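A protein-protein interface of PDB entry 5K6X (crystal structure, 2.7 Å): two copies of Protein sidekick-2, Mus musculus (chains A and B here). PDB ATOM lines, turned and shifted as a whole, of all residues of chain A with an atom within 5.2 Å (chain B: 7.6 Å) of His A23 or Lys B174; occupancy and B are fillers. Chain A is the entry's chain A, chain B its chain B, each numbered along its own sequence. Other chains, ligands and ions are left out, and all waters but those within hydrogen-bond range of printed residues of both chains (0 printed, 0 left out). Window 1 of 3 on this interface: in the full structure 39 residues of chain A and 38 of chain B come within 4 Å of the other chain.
The side-chain amide oxygen (OE1) of Gln A21 sits at hydrogen-bond distance from a ring nitrogen (NE2) of His A23, 2.7 Å away.
The backbone NH (N) of His A23 is in hydrogen-bond range of the backbone carbonyl oxygen (O) of Gln A93, 2.8 Å away.
O of His A23 is in hydrogen-bond range of N of Ala A95 (2.7 Å).
N of Lys B174 sits at hydrogen-bond distance from OD1 of Asn B172, at 3.0 Å.
OD1 of Asn B172 lies within hydrogen-bond range of N of Asn B175, at 3.0 Å.
OD1 of Asn B175 sits at hydrogen-bond distance from N of Asp B177 (2.9 Å).
Printed residues of chain B that touch a printed residue of chain A: Leu B24, Arg B28, Asp B173, Lys B174 and Asn B175.
Hydrophobic or aromatic side chains of chain B that line the printed part of chain A: Leu B24.
Among the printed residues, 6 pairs touch across the chains.
Among the printed residues, no Asp or Glu carboxylate lies within 4 Å of a Lys or Arg side-chain nitrogen of the other chain.
The side-chain hydroxyl (OG1) of Thr A32 lies within hydrogen-bond range of the backbone carbonyl oxygen (O) of Asp B173, at 2.7 Å.
O of Lys B174 sits close to O of Val A30 (3.5 Å).
Among the printed residues, merely in contact across the chains: His A23 with Lys B174, Leu A24 with Arg B28, Val A30 with Leu B24 and Val A30 with Asn B175.
Positions printed for both chains: 22, 23, 24, 25, 93, 94 and 95.
Of the 6 pairs that touch across the chains among the printed residues, none has its exchanged pair printed and touching as well.
Val A22 touches none of the printed residues of chain B.
His A23 touches just one residue of chain B: Lys B174.
Printed residues of chain B within 4 Å of Thr A32: Asp B173.
Of chain A, only His A23 and Val A30 come within 4 Å of Lys B174.
Printed residues of chain A within 4 Å of Asn B175: Val A30 (3.6 Å).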
ATOM      1  N   GLN A  21      -8.030 -16.385 -23.664  1.00  0.00           N
ATOM      2  CA  GLN A  21      -7.402 -16.632 -22.369  1.00  0.00           C
ATOM      3  C   GLN A  21      -8.195 -17.649 -21.554  1.00  0.00           C
ATOM      4  O   GLN A  21      -9.416 -17.554 -21.435  1.00  0.00           O
ATOM      5  CB  GLN A  21      -7.249 -15.323 -21.587  1.00  0.00           C
ATOM      6  CG  GLN A  21      -8.533 -14.522 -21.441  1.00  0.00           C
ATOM      7  CD  GLN A  21      -8.299 -13.150 -20.839  1.00  0.00           C
ATOM      8  OE1 GLN A  21      -7.953 -13.026 -19.664  1.00  0.00           O
ATOM      9  NE2 GLN A  21      -8.491 -12.109 -21.643  1.00  0.00           N
ATOM     10  N   VAL A  22      -7.489 -18.633 -21.005  1.00  0.00           N
ATOM     11  CA  VAL A  22      -8.123 -19.690 -20.228  1.00  0.00           C
ATOM     12  C   VAL A  22      -7.909 -19.471 -18.733  1.00  0.00           C
ATOM     13  O   VAL A  22      -6.803 -19.152 -18.294  1.00  0.00           O
ATOM     14  CB  VAL A  22      -7.583 -21.079 -20.629  1.00  0.00           C
ATOM     15  CG1 VAL A  22      -8.269 -22.177 -19.829  1.00  0.00           C
ATOM     16  CG2 VAL A  22      -7.773 -21.304 -22.117  1.00  0.00           C
ATOM     17  N   HIS A  23      -8.976 -19.636 -17.956  1.00  0.00           N
ATOM     18  CA  HIS A  23      -8.903 -19.455 -16.510  1.00  0.00           C
ATOM     19  C   HIS A  23      -9.639 -20.561 -15.762  1.00  0.00           C
ATOM     20  O   HIS A  23     -10.573 -21.160 -16.287  1.00  0.00           O
ATOM     21  CB  HIS A  23      -9.473 -18.089 -16.115  1.00  0.00           C
ATOM     22  CG  HIS A  23      -8.820 -16.936 -16.811  1.00  0.00           C
ATOM     23  ND1 HIS A  23      -7.627 -16.389 -16.386  1.00  0.00           N
ATOM     24  CD2 HIS A  23      -9.190 -16.225 -17.902  1.00  0.00           C
ATOM     25  CE1 HIS A  23      -7.293 -15.391 -17.183  1.00  0.00           C
ATOM     26  NE2 HIS A  23      -8.224 -15.271 -18.114  1.00  0.00           N
ATOM     27  N   LEU A  24      -9.211 -20.823 -14.530  1.00  0.00           N
ATOM     28  CA  LEU A  24      -9.863 -21.814 -13.679  1.00  0.00           C
ATOM     29  C   LEU A  24     -11.080 -21.235 -12.967  1.00  0.00           C
ATOM     30  O   LEU A  24     -11.125 -20.040 -12.671  1.00  0.00           O
ATOM     31  CB  LEU A  24      -8.882 -22.363 -12.640  1.00  0.00           C
ATOM     32  CG  LEU A  24      -7.669 -23.165 -13.113  1.00  0.00           C
ATOM     33  CD1 LEU A  24      -6.961 -23.797 -11.923  1.00  0.00           C
ATOM     34  CD2 LEU A  24      -8.082 -24.228 -14.117  1.00  0.00           C
ATOM     35  N   GLU A  25     -12.066 -22.086 -12.697  1.00  0.00           N
ATOM     36  CA  GLU A  25     -13.182 -21.710 -11.838  1.00  0.00           C
ATOM     37  C   GLU A  25     -12.690 -21.303 -10.450  1.00  0.00           C
ATOM     38  O   GLU A  25     -11.830 -21.967  -9.869  1.00  0.00           O
ATOM     39  CB  GLU A  25     -14.190 -22.855 -11.715  1.00  0.00           C
ATOM     40  CG  GLU A  25     -15.479 -22.635 -12.482  1.00  0.00           C
ATOM     41  CD  GLU A  25     -16.372 -23.861 -12.485  1.00  0.00           C
ATOM     42  OE1 GLU A  25     -15.897 -24.946 -12.089  1.00  0.00           O
ATOM     43  OE2 GLU A  25     -17.552 -23.738 -12.880  1.00  0.00           O
ATOM     44  N   LEU A  29     -10.403 -12.755 -12.122  1.00  0.00           N
ATOM     45  CA  LEU A  29     -10.077 -12.203 -13.429  1.00  0.00           C
ATOM     46  C   LEU A  29     -10.036 -10.683 -13.377  1.00  0.00           C
ATOM     47  O   LEU A  29     -10.944 -10.045 -12.843  1.00  0.00           O
ATOM     48  CB  LEU A  29     -11.093 -12.666 -14.475  1.00  0.00           C
ATOM     49  CG  LEU A  29     -10.918 -12.103 -15.884  1.00  0.00           C
ATOM     50  CD1 LEU A  29      -9.682 -12.689 -16.543  1.00  0.00           C
ATOM     51  CD2 LEU A  29     -12.161 -12.361 -16.728  1.00  0.00           C
ATOM     52  N   VAL A  30      -8.977 -10.105 -13.931  1.00  0.00           N
ATOM     53  CA  VAL A  30      -8.877  -8.657 -14.039  1.00  0.00           C
ATOM     54  C   VAL A  30      -8.704  -8.248 -15.497  1.00  0.00           C
ATOM     55  O   VAL A  30      -7.633  -8.412 -16.081  1.00  0.00           O
ATOM     56  CB  VAL A  30      -7.704  -8.097 -13.212  1.00  0.00           C
ATOM     57  CG1 VAL A  30      -7.663  -6.583 -13.321  1.00  0.00           C
ATOM     58  CG2 VAL A  30      -7.820  -8.524 -11.757  1.00  0.00           C
ATOM     59  N   THR A  32      -8.529  -5.262 -18.296  1.00  0.00           N
ATOM     60  CA  THR A  32      -8.125  -3.864 -18.329  1.00  0.00           C
ATOM     61  C   THR A  32      -8.370  -3.230 -19.692  1.00  0.00           C
ATOM     62  O   THR A  32      -8.190  -3.868 -20.730  1.00  0.00           O
ATOM     63  CB  THR A  32      -6.637  -3.704 -17.968  1.00  0.00           C
ATOM     64  OG1 THR A  32      -5.836  -4.446 -18.897  1.00  0.00           O
ATOM     65  CG2 THR A  32      -6.371  -4.209 -16.557  1.00  0.00           C
ATOM     66  N   LEU A  66     -14.508 -16.649 -10.774  1.00  0.00           N
ATOM     67  CA  LEU A  66     -15.016 -17.071 -12.075  1.00  0.00           C
ATOM     68  C   LEU A  66     -15.806 -18.374 -12.006  1.00  0.00           C
ATOM     69  O   LEU A  66     -15.407 -19.320 -11.326  1.00  0.00           O
ATOM     70  CB  LEU A  66     -13.860 -17.227 -13.066  1.00  0.00           C
ATOM     71  CG  LEU A  66     -13.280 -15.942 -13.656  1.00  0.00           C
ATOM     72  CD1 LEU A  66     -11.951 -16.224 -14.333  1.00  0.00           C
ATOM     73  CD2 LEU A  66     -14.255 -15.306 -14.637  1.00  0.00           C
ATOM     74  N   VAL A  92     -12.824 -14.948 -22.866  1.00  0.00           N
ATOM     75  CA  VAL A  92     -12.488 -15.580 -21.601  1.00  0.00           C
ATOM     76  C   VAL A  92     -13.074 -16.986 -21.562  1.00  0.00           C
ATOM     77  O   VAL A  92     -14.290 -17.168 -21.645  1.00  0.00           O
ATOM     78  CB  VAL A  92     -13.000 -14.767 -20.402  1.00  0.00           C
ATOM     79  CG1 VAL A  92     -12.845 -15.562 -19.119  1.00  0.00           C
ATOM     80  CG2 VAL A  92     -12.255 -13.444 -20.306  1.00  0.00           C
ATOM     81  N   GLN A  93     -12.200 -17.977 -21.441  1.00  0.00           N
ATOM     82  CA  GLN A  93     -12.624 -19.368 -21.383  1.00  0.00           C
ATOM     83  C   GLN A  93     -12.380 -19.919 -19.988  1.00  0.00           C
ATOM     84  O   GLN A  93     -11.296 -19.754 -19.429  1.00  0.00           O
ATOM     85  CB  GLN A  93     -11.884 -20.204 -22.427  1.00  0.00           C
ATOM     86  CG  GLN A  93     -12.102 -19.747 -23.859  1.00  0.00           C
ATOM     87  CD  GLN A  93     -11.302 -20.564 -24.854  1.00  0.00           C
ATOM     88  OE1 GLN A  93     -10.124 -20.847 -24.637  1.00  0.00           O
ATOM     89  NE2 GLN A  93     -11.941 -20.948 -25.953  1.00  0.00           N
ATOM     90  N   VAL A  94     -13.391 -20.570 -19.425  1.00  0.00           N
ATOM     91  CA  VAL A  94     -13.289 -21.085 -18.067  1.00  0.00           C
ATOM     92  C   VAL A  94     -13.139 -22.601 -18.050  1.00  0.00           C
ATOM     93  O   VAL A  94     -13.997 -23.327 -18.554  1.00  0.00           O
ATOM     94  CB  VAL A  94     -14.515 -20.692 -17.223  1.00  0.00           C
ATOM     95  CG1 VAL A  94     -14.374 -21.226 -15.807  1.00  0.00           C
ATOM     96  CG2 VAL A  94     -14.692 -19.182 -17.216  1.00  0.00           C
ATOM     97  N   ALA A  95     -12.038 -23.069 -17.469  1.00  0.00           N
ATOM     98  CA  ALA A  95     -11.790 -24.496 -17.334  1.00  0.00           C
ATOM     99  C   ALA A  95     -12.710 -25.104 -16.283  1.00  0.00           C
ATOM    100  O   ALA A  95     -12.723 -24.674 -15.129  1.00  0.00           O
ATOM    101  CB  ALA A  95     -10.335 -24.752 -16.979  1.00  0.00           C
ATOM    102  N   VAL B  22       0.483 -17.502 -18.014  1.00  0.00           N
ATOM    103  CA  VAL B  22       0.516 -16.354 -17.114  1.00  0.00           C
ATOM    104  C   VAL B  22      -0.623 -16.447 -16.102  1.00  0.00           C
ATOM    105  O   VAL B  22      -1.760 -16.754 -16.463  1.00  0.00           O
ATOM    106  CB  VAL B  22       0.416 -15.021 -17.887  1.00  0.00           C
ATOM    107  CG1 VAL B  22       0.473 -13.841 -16.930  1.00  0.00           C
ATOM    108  CG2 VAL B  22       1.527 -14.922 -18.919  1.00  0.00           C
ATOM    109  N   HIS B  23      -0.315 -16.185 -14.837  1.00  0.00           N
ATOM    110  CA  HIS B  23      -1.319 -16.266 -13.784  1.00  0.00           C
ATOM    111  C   HIS B  23      -1.237 -15.083 -12.823  1.00  0.00           C
ATOM    112  O   HIS B  23      -0.180 -14.472 -12.663  1.00  0.00           O
ATOM    113  CB  HIS B  23      -1.161 -17.574 -13.009  1.00  0.00           C
ATOM    114  CG  HIS B  23      -1.170 -18.794 -13.875  1.00  0.00           C
ATOM    115  ND1 HIS B  23      -2.333 -19.378 -14.329  1.00  0.00           N
ATOM    116  CD2 HIS B  23      -0.156 -19.544 -14.368  1.00  0.00           C
ATOM    117  CE1 HIS B  23      -2.036 -20.432 -15.066  1.00  0.00           C
ATOM    118  NE2 HIS B  23      -0.720 -20.555 -15.105  1.00  0.00           N
ATOM    119  N   LEU B  24      -2.359 -14.766 -12.184  1.00  0.00           N
ATOM    120  CA  LEU B  24      -2.388 -13.700 -11.189  1.00  0.00           C
ATOM    121  C   LEU B  24      -1.920 -14.193  -9.827  1.00  0.00           C
ATOM    122  O   LEU B  24      -2.097 -15.362  -9.483  1.00  0.00           O
ATOM    123  CB  LEU B  24      -3.795 -13.113 -11.059  1.00  0.00           C
ATOM    124  CG  LEU B  24      -4.382 -12.379 -12.262  1.00  0.00           C
ATOM    125  CD1 LEU B  24      -5.667 -11.684 -11.860  1.00  0.00           C
ATOM    126  CD2 LEU B  24      -3.383 -11.378 -12.809  1.00  0.00           C
ATOM    127  N   GLU B  25      -1.314 -13.293  -9.062  1.00  0.00           N
ATOM    128  CA  GLU B  25      -0.994 -13.557  -7.667  1.00  0.00           C
ATOM    129  C   GLU B  25      -2.268 -13.874  -6.892  1.00  0.00           C
ATOM    130  O   GLU B  25      -3.281 -13.193  -7.049  1.00  0.00           O
ATOM    131  CB  GLU B  25      -0.275 -12.356  -7.050  1.00  0.00           C
ATOM    132  CG  GLU B  25       1.213 -12.558  -6.841  1.00  0.00           C
ATOM    133  CD  GLU B  25       1.920 -11.279  -6.425  1.00  0.00           C
ATOM    134  OE1 GLU B  25       1.298 -10.198  -6.519  1.00  0.00           O
ATOM    135  OE2 GLU B  25       3.096 -11.356  -6.006  1.00  0.00           O
ATOM    136  N   ASN B  27      -4.130 -16.412  -7.256  1.00  0.00           N
ATOM    137  CA  ASN B  27      -4.911 -17.376  -8.026  1.00  0.00           C
ATOM    138  C   ASN B  27      -4.370 -18.796  -7.878  1.00  0.00           C
ATOM    139  O   ASN B  27      -3.218 -18.999  -7.490  1.00  0.00           O
ATOM    140  CB  ASN B  27      -4.951 -16.978  -9.502  1.00  0.00           C
ATOM    141  CG  ASN B  27      -6.175 -16.147  -9.847  1.00  0.00           C
ATOM    142  OD1 ASN B  27      -7.008 -15.862  -8.989  1.00  0.00           O
ATOM    143  ND2 ASN B  27      -6.289 -15.759 -11.111  1.00  0.00           N
ATOM    144  N   ARG B  28      -5.212 -19.777  -8.186  1.00  0.00           N
ATOM    145  CA  ARG B  28      -4.844 -21.180  -8.034  1.00  0.00           C
ATOM    146  C   ARG B  28      -4.230 -21.758  -9.307  1.00  0.00           C
ATOM    147  O   ARG B  28      -4.715 -21.513 -10.411  1.00  0.00           O
ATOM    148  CB  ARG B  28      -6.075 -21.995  -7.633  1.00  0.00           C
ATOM    149  CG  ARG B  28      -5.882 -23.499  -7.657  1.00  0.00           C
ATOM    150  CD  ARG B  28      -7.204 -24.208  -7.423  1.00  0.00           C
ATOM    151  NE  ARG B  28      -7.075 -25.663  -7.455  1.00  0.00           N
ATOM    152  CZ  ARG B  28      -6.840 -26.415  -6.385  1.00  0.00           C
ATOM    153  NH1 ARG B  28      -6.705 -25.852  -5.192  1.00  0.00           N
ATOM    154  NH2 ARG B  28      -6.738 -27.731  -6.508  1.00  0.00           N
ATOM    155  N   GLN B  93       4.395 -18.101 -15.331  1.00  0.00           N
ATOM    156  CA  GLN B  93       4.707 -16.697 -15.107  1.00  0.00           C
ATOM    157  C   GLN B  93       3.654 -16.036 -14.227  1.00  0.00           C
ATOM    158  O   GLN B  93       2.455 -16.167 -14.470  1.00  0.00           O
ATOM    159  CB  GLN B  93       4.828 -15.963 -16.442  1.00  0.00           C
ATOM    160  CG  GLN B  93       5.921 -16.517 -17.341  1.00  0.00           C
ATOM    161  CD  GLN B  93       5.979 -15.823 -18.684  1.00  0.00           C
ATOM    162  OE1 GLN B  93       4.951 -15.589 -19.318  1.00  0.00           O
ATOM    163  NE2 GLN B  93       7.186 -15.482 -19.123  1.00  0.00           N
ATOM    164  N   VAL B  94       4.112 -15.326 -13.201  1.00  0.00           N
ATOM    165  CA  VAL B  94       3.215 -14.689 -12.245  1.00  0.00           C
ATOM    166  C   VAL B  94       3.175 -13.179 -12.447  1.00  0.00           C
ATOM    167  O   VAL B  94       4.203 -12.507 -12.372  1.00  0.00           O
ATOM    168  CB  VAL B  94       3.628 -14.996 -10.793  1.00  0.00           C
ATOM    169  CG1 VAL B  94       2.674 -14.325  -9.817  1.00  0.00           C
ATOM    170  CG2 VAL B  94       3.674 -16.499 -10.565  1.00  0.00           C
ATOM    171  N   ALA B  95       1.980 -12.655 -12.700  1.00  0.00           N
ATOM    172  CA  ALA B  95       1.791 -11.221 -12.872  1.00  0.00           C
ATOM    173  C   ALA B  95       1.949 -10.485 -11.550  1.00  0.00           C
ATOM    174  O   ALA B  95       1.263 -10.785 -10.571  1.00  0.00           O
ATOM    175  CB  ALA B  95       0.432 -10.935 -13.471  1.00  0.00           C
ATOM    176  N   TYR B  96       2.855  -9.515 -11.531  1.00  0.00           N
ATOM    177  CA  TYR B  96       3.129  -8.742 -10.331  1.00  0.00           C
ATOM    178  C   TYR B  96       3.573  -7.338 -10.708  1.00  0.00           C
ATOM    179  O   TYR B  96       3.811  -7.046 -11.881  1.00  0.00           O
ATOM    180  CB  TYR B  96       4.215  -9.414  -9.487  1.00  0.00           C
ATOM    181  CG  TYR B  96       5.607  -9.242 -10.060  1.00  0.00           C
ATOM    182  CD1 TYR B  96       6.446  -8.227  -9.608  1.00  0.00           C
ATOM    183  CD2 TYR B  96       6.079 -10.084 -11.059  1.00  0.00           C
ATOM    184  CE1 TYR B  96       7.714  -8.059 -10.130  1.00  0.00           C
ATOM    185  CE2 TYR B  96       7.349  -9.921 -11.590  1.00  0.00           C
ATOM    186  CZ  TYR B  96       8.160  -8.908 -11.120  1.00  0.00           C
ATOM    187  OH  TYR B  96       9.422  -8.743 -11.641  1.00  0.00           O
ATOM    188  N   PHE B 125       5.886  -7.754 -14.131  1.00  0.00           N
ATOM    189  CA  PHE B 125       5.579  -8.640 -15.246  1.00  0.00           C
ATOM    190  C   PHE B 125       4.075  -8.692 -15.489  1.00  0.00           C
ATOM    191  O   PHE B 125       3.305  -8.924 -14.558  1.00  0.00           O
ATOM    192  CB  PHE B 125       6.110 -10.053 -15.015  1.00  0.00           C
ATOM    193  CG  PHE B 125       5.838 -10.976 -16.164  1.00  0.00           C
ATOM    194  CD1 PHE B 125       6.668 -10.983 -17.272  1.00  0.00           C
ATOM    195  CD2 PHE B 125       4.729 -11.805 -16.157  1.00  0.00           C
ATOM    196  CE1 PHE B 125       6.410 -11.815 -18.341  1.00  0.00           C
ATOM    197  CE2 PHE B 125       4.464 -12.635 -17.225  1.00  0.00           C
ATOM    198  CZ  PHE B 125       5.306 -12.642 -18.317  1.00  0.00           C
ATOM    199  N   PRO B 126       3.650  -8.469 -16.744  1.00  0.00           N
ATOM    200  CA  PRO B 126       4.508  -8.093 -17.876  1.00  0.00           C
ATOM    201  C   PRO B 126       4.974  -6.645 -17.785  1.00  0.00           C
ATOM    202  O   PRO B 126       4.634  -5.972 -16.811  1.00  0.00           O
ATOM    203  CB  PRO B 126       3.595  -8.292 -19.087  1.00  0.00           C
ATOM    204  CG  PRO B 126       2.229  -8.053 -18.551  1.00  0.00           C
ATOM    205  CD  PRO B 126       2.243  -8.621 -17.156  1.00  0.00           C
ATOM    206  N   ARG B 127       5.740  -6.180 -18.767  1.00  0.00           N
ATOM    207  CA  ARG B 127       6.162  -4.785 -18.780  1.00  0.00           C
ATOM    208  C   ARG B 127       4.927  -3.890 -18.750  1.00  0.00           C
ATOM    209  O   ARG B 127       3.980  -4.105 -19.508  1.00  0.00           O
ATOM    210  CB  ARG B 127       7.017  -4.476 -20.013  1.00  0.00           C
ATOM    211  CG  ARG B 127       7.670  -3.099 -19.979  1.00  0.00           C
ATOM    212  CD  ARG B 127       7.956  -2.557 -21.367  1.00  0.00           C
ATOM    213  NE  ARG B 127       8.991  -3.315 -22.064  1.00  0.00           N
ATOM    214  CZ  ARG B 127      10.294  -3.079 -21.946  1.00  0.00           C
ATOM    215  NH1 ARG B 127      11.168  -3.816 -22.620  1.00  0.00           N
ATOM    216  NH2 ARG B 127      10.724  -2.110 -21.150  1.00  0.00           N
ATOM    217  N   PRO B 128       4.935  -2.877 -17.870  1.00  0.00           N
ATOM    218  CA  PRO B 128       3.740  -2.043 -17.706  1.00  0.00           C
ATOM    219  C   PRO B 128       3.579  -1.015 -18.816  1.00  0.00           C
ATOM    220  O   PRO B 128       4.550  -0.649 -19.479  1.00  0.00           O
ATOM    221  CB  PRO B 128       3.971  -1.351 -16.365  1.00  0.00           C
ATOM    222  CG  PRO B 128       5.446  -1.343 -16.181  1.00  0.00           C
ATOM    223  CD  PRO B 128       6.021  -2.501 -16.947  1.00  0.00           C
ATOM    224  N   VAL B 171       1.042   1.296 -15.459  1.00  0.00           N
ATOM    225  CA  VAL B 171      -0.059   0.383 -15.187  1.00  0.00           C
ATOM    226  C   VAL B 171       0.235  -1.021 -15.706  1.00  0.00           C
ATOM    227  O   VAL B 171       0.638  -1.200 -16.856  1.00  0.00           O
ATOM    228  CB  VAL B 171      -1.372   0.888 -15.812  1.00  0.00           C
ATOM    229  CG1 VAL B 171      -2.514  -0.058 -15.478  1.00  0.00           C
ATOM    230  CG2 VAL B 171      -1.690   2.289 -15.311  1.00  0.00           C
ATOM    231  N   ASN B 172       0.040  -2.012 -14.842  1.00  0.00           N
ATOM    232  CA  ASN B 172       0.172  -3.412 -15.228  1.00  0.00           C
ATOM    233  C   ASN B 172      -1.129  -3.922 -15.838  1.00  0.00           C
ATOM    234  O   ASN B 172      -2.129  -4.080 -15.142  1.00  0.00           O
ATOM    235  CB  ASN B 172       0.573  -4.258 -14.017  1.00  0.00           C
ATOM    236  CG  ASN B 172       0.863  -5.701 -14.377  1.00  0.00           C
ATOM    237  OD1 ASN B 172      -0.045  -6.475 -14.685  1.00  0.00           O
ATOM    238  ND2 ASN B 172       2.136  -6.074 -14.334  1.00  0.00           N
ATOM    239  N   ASP B 173      -1.107  -4.179 -17.142  1.00  0.00           N
ATOM    240  CA  ASP B 173      -2.323  -4.519 -17.878  1.00  0.00           C
ATOM    241  C   ASP B 173      -2.926  -5.865 -17.487  1.00  0.00           C
ATOM    242  O   ASP B 173      -4.066  -6.159 -17.843  1.00  0.00           O
ATOM    243  CB  ASP B 173      -2.050  -4.510 -19.383  1.00  0.00           C
ATOM    244  CG  ASP B 173      -0.841  -5.341 -19.762  1.00  0.00           C
ATOM    245  OD1 ASP B 173       0.289  -4.929 -19.427  1.00  0.00           O
ATOM    246  OD2 ASP B 173      -1.018  -6.408 -20.388  1.00  0.00           O
ATOM    247  N   LYS B 174      -2.167  -6.683 -16.766  1.00  0.00           N
ATOM    248  CA  LYS B 174      -2.646  -8.007 -16.381  1.00  0.00           C
ATOM    249  C   LYS B 174      -3.375  -8.027 -15.034  1.00  0.00           C
ATOM    250  O   LYS B 174      -4.391  -8.708 -14.893  1.00  0.00           O
ATOM    251  CB  LYS B 174      -1.479  -9.000 -16.358  1.00  0.00           C
ATOM    252  CG  LYS B 174      -1.880 -10.426 -16.016  1.00  0.00           C
ATOM    253  CD  LYS B 174      -2.845 -11.016 -17.030  1.00  0.00           C
ATOM    254  CE  LYS B 174      -3.214 -12.446 -16.656  1.00  0.00           C
ATOM    255  NZ  LYS B 174      -4.172 -13.061 -17.616  1.00  0.00           N
ATOM    256  N   ASN B 175      -2.871  -7.285 -14.051  1.00  0.00           N
ATOM    257  CA  ASN B 175      -3.523  -7.242 -12.742  1.00  0.00           C
ATOM    258  C   ASN B 175      -4.099  -5.871 -12.385  1.00  0.00           C
ATOM    259  O   ASN B 175      -4.733  -5.707 -11.343  1.00  0.00           O
ATOM    260  CB  ASN B 175      -2.553  -7.702 -11.643  1.00  0.00           C
ATOM    261  CG  ASN B 175      -1.330  -6.808 -11.514  1.00  0.00           C
ATOM    262  OD1 ASN B 175      -1.292  -5.699 -12.043  1.00  0.00           O
ATOM    263  ND2 ASN B 175      -0.321  -7.291 -10.797  1.00  0.00           N
ATOM    264  N   GLY B 176      -3.880  -4.892 -13.255  1.00  0.00           N
ATOM    265  CA  GLY B 176      -4.429  -3.563 -13.060  1.00  0.00           C
ATOM    266  C   GLY B 176      -3.741  -2.726 -11.993  1.00  0.00           C
ATOM    267  O   GLY B 176      -4.321  -1.763 -11.492  1.00  0.00           O
ATOM    268  N   ASP B 177      -2.508  -3.082 -11.644  1.00  0.00           N
ATOM    269  CA  ASP B 177      -1.730  -2.291 -10.693  1.00  0.00           C
ATOM    270  C   ASP B 177      -1.369  -0.935 -11.289  1.00  0.00           C
ATOM    271  O   ASP B 177      -1.018  -0.838 -12.464  1.00  0.00           O
ATOM    272  CB  ASP B 177      -0.459  -3.035 -10.275  1.00  0.00           C
ATOM    273  CG  ASP B 177      -0.704  -4.031  -9.160  1.00  0.00           C
ATOM    274  OD1 ASP B 177      -1.767  -3.948  -8.513  1.00  0.00           O
ATOM    275  OD2 ASP B 177       0.165  -4.899  -8.931  1.00  0.00           O
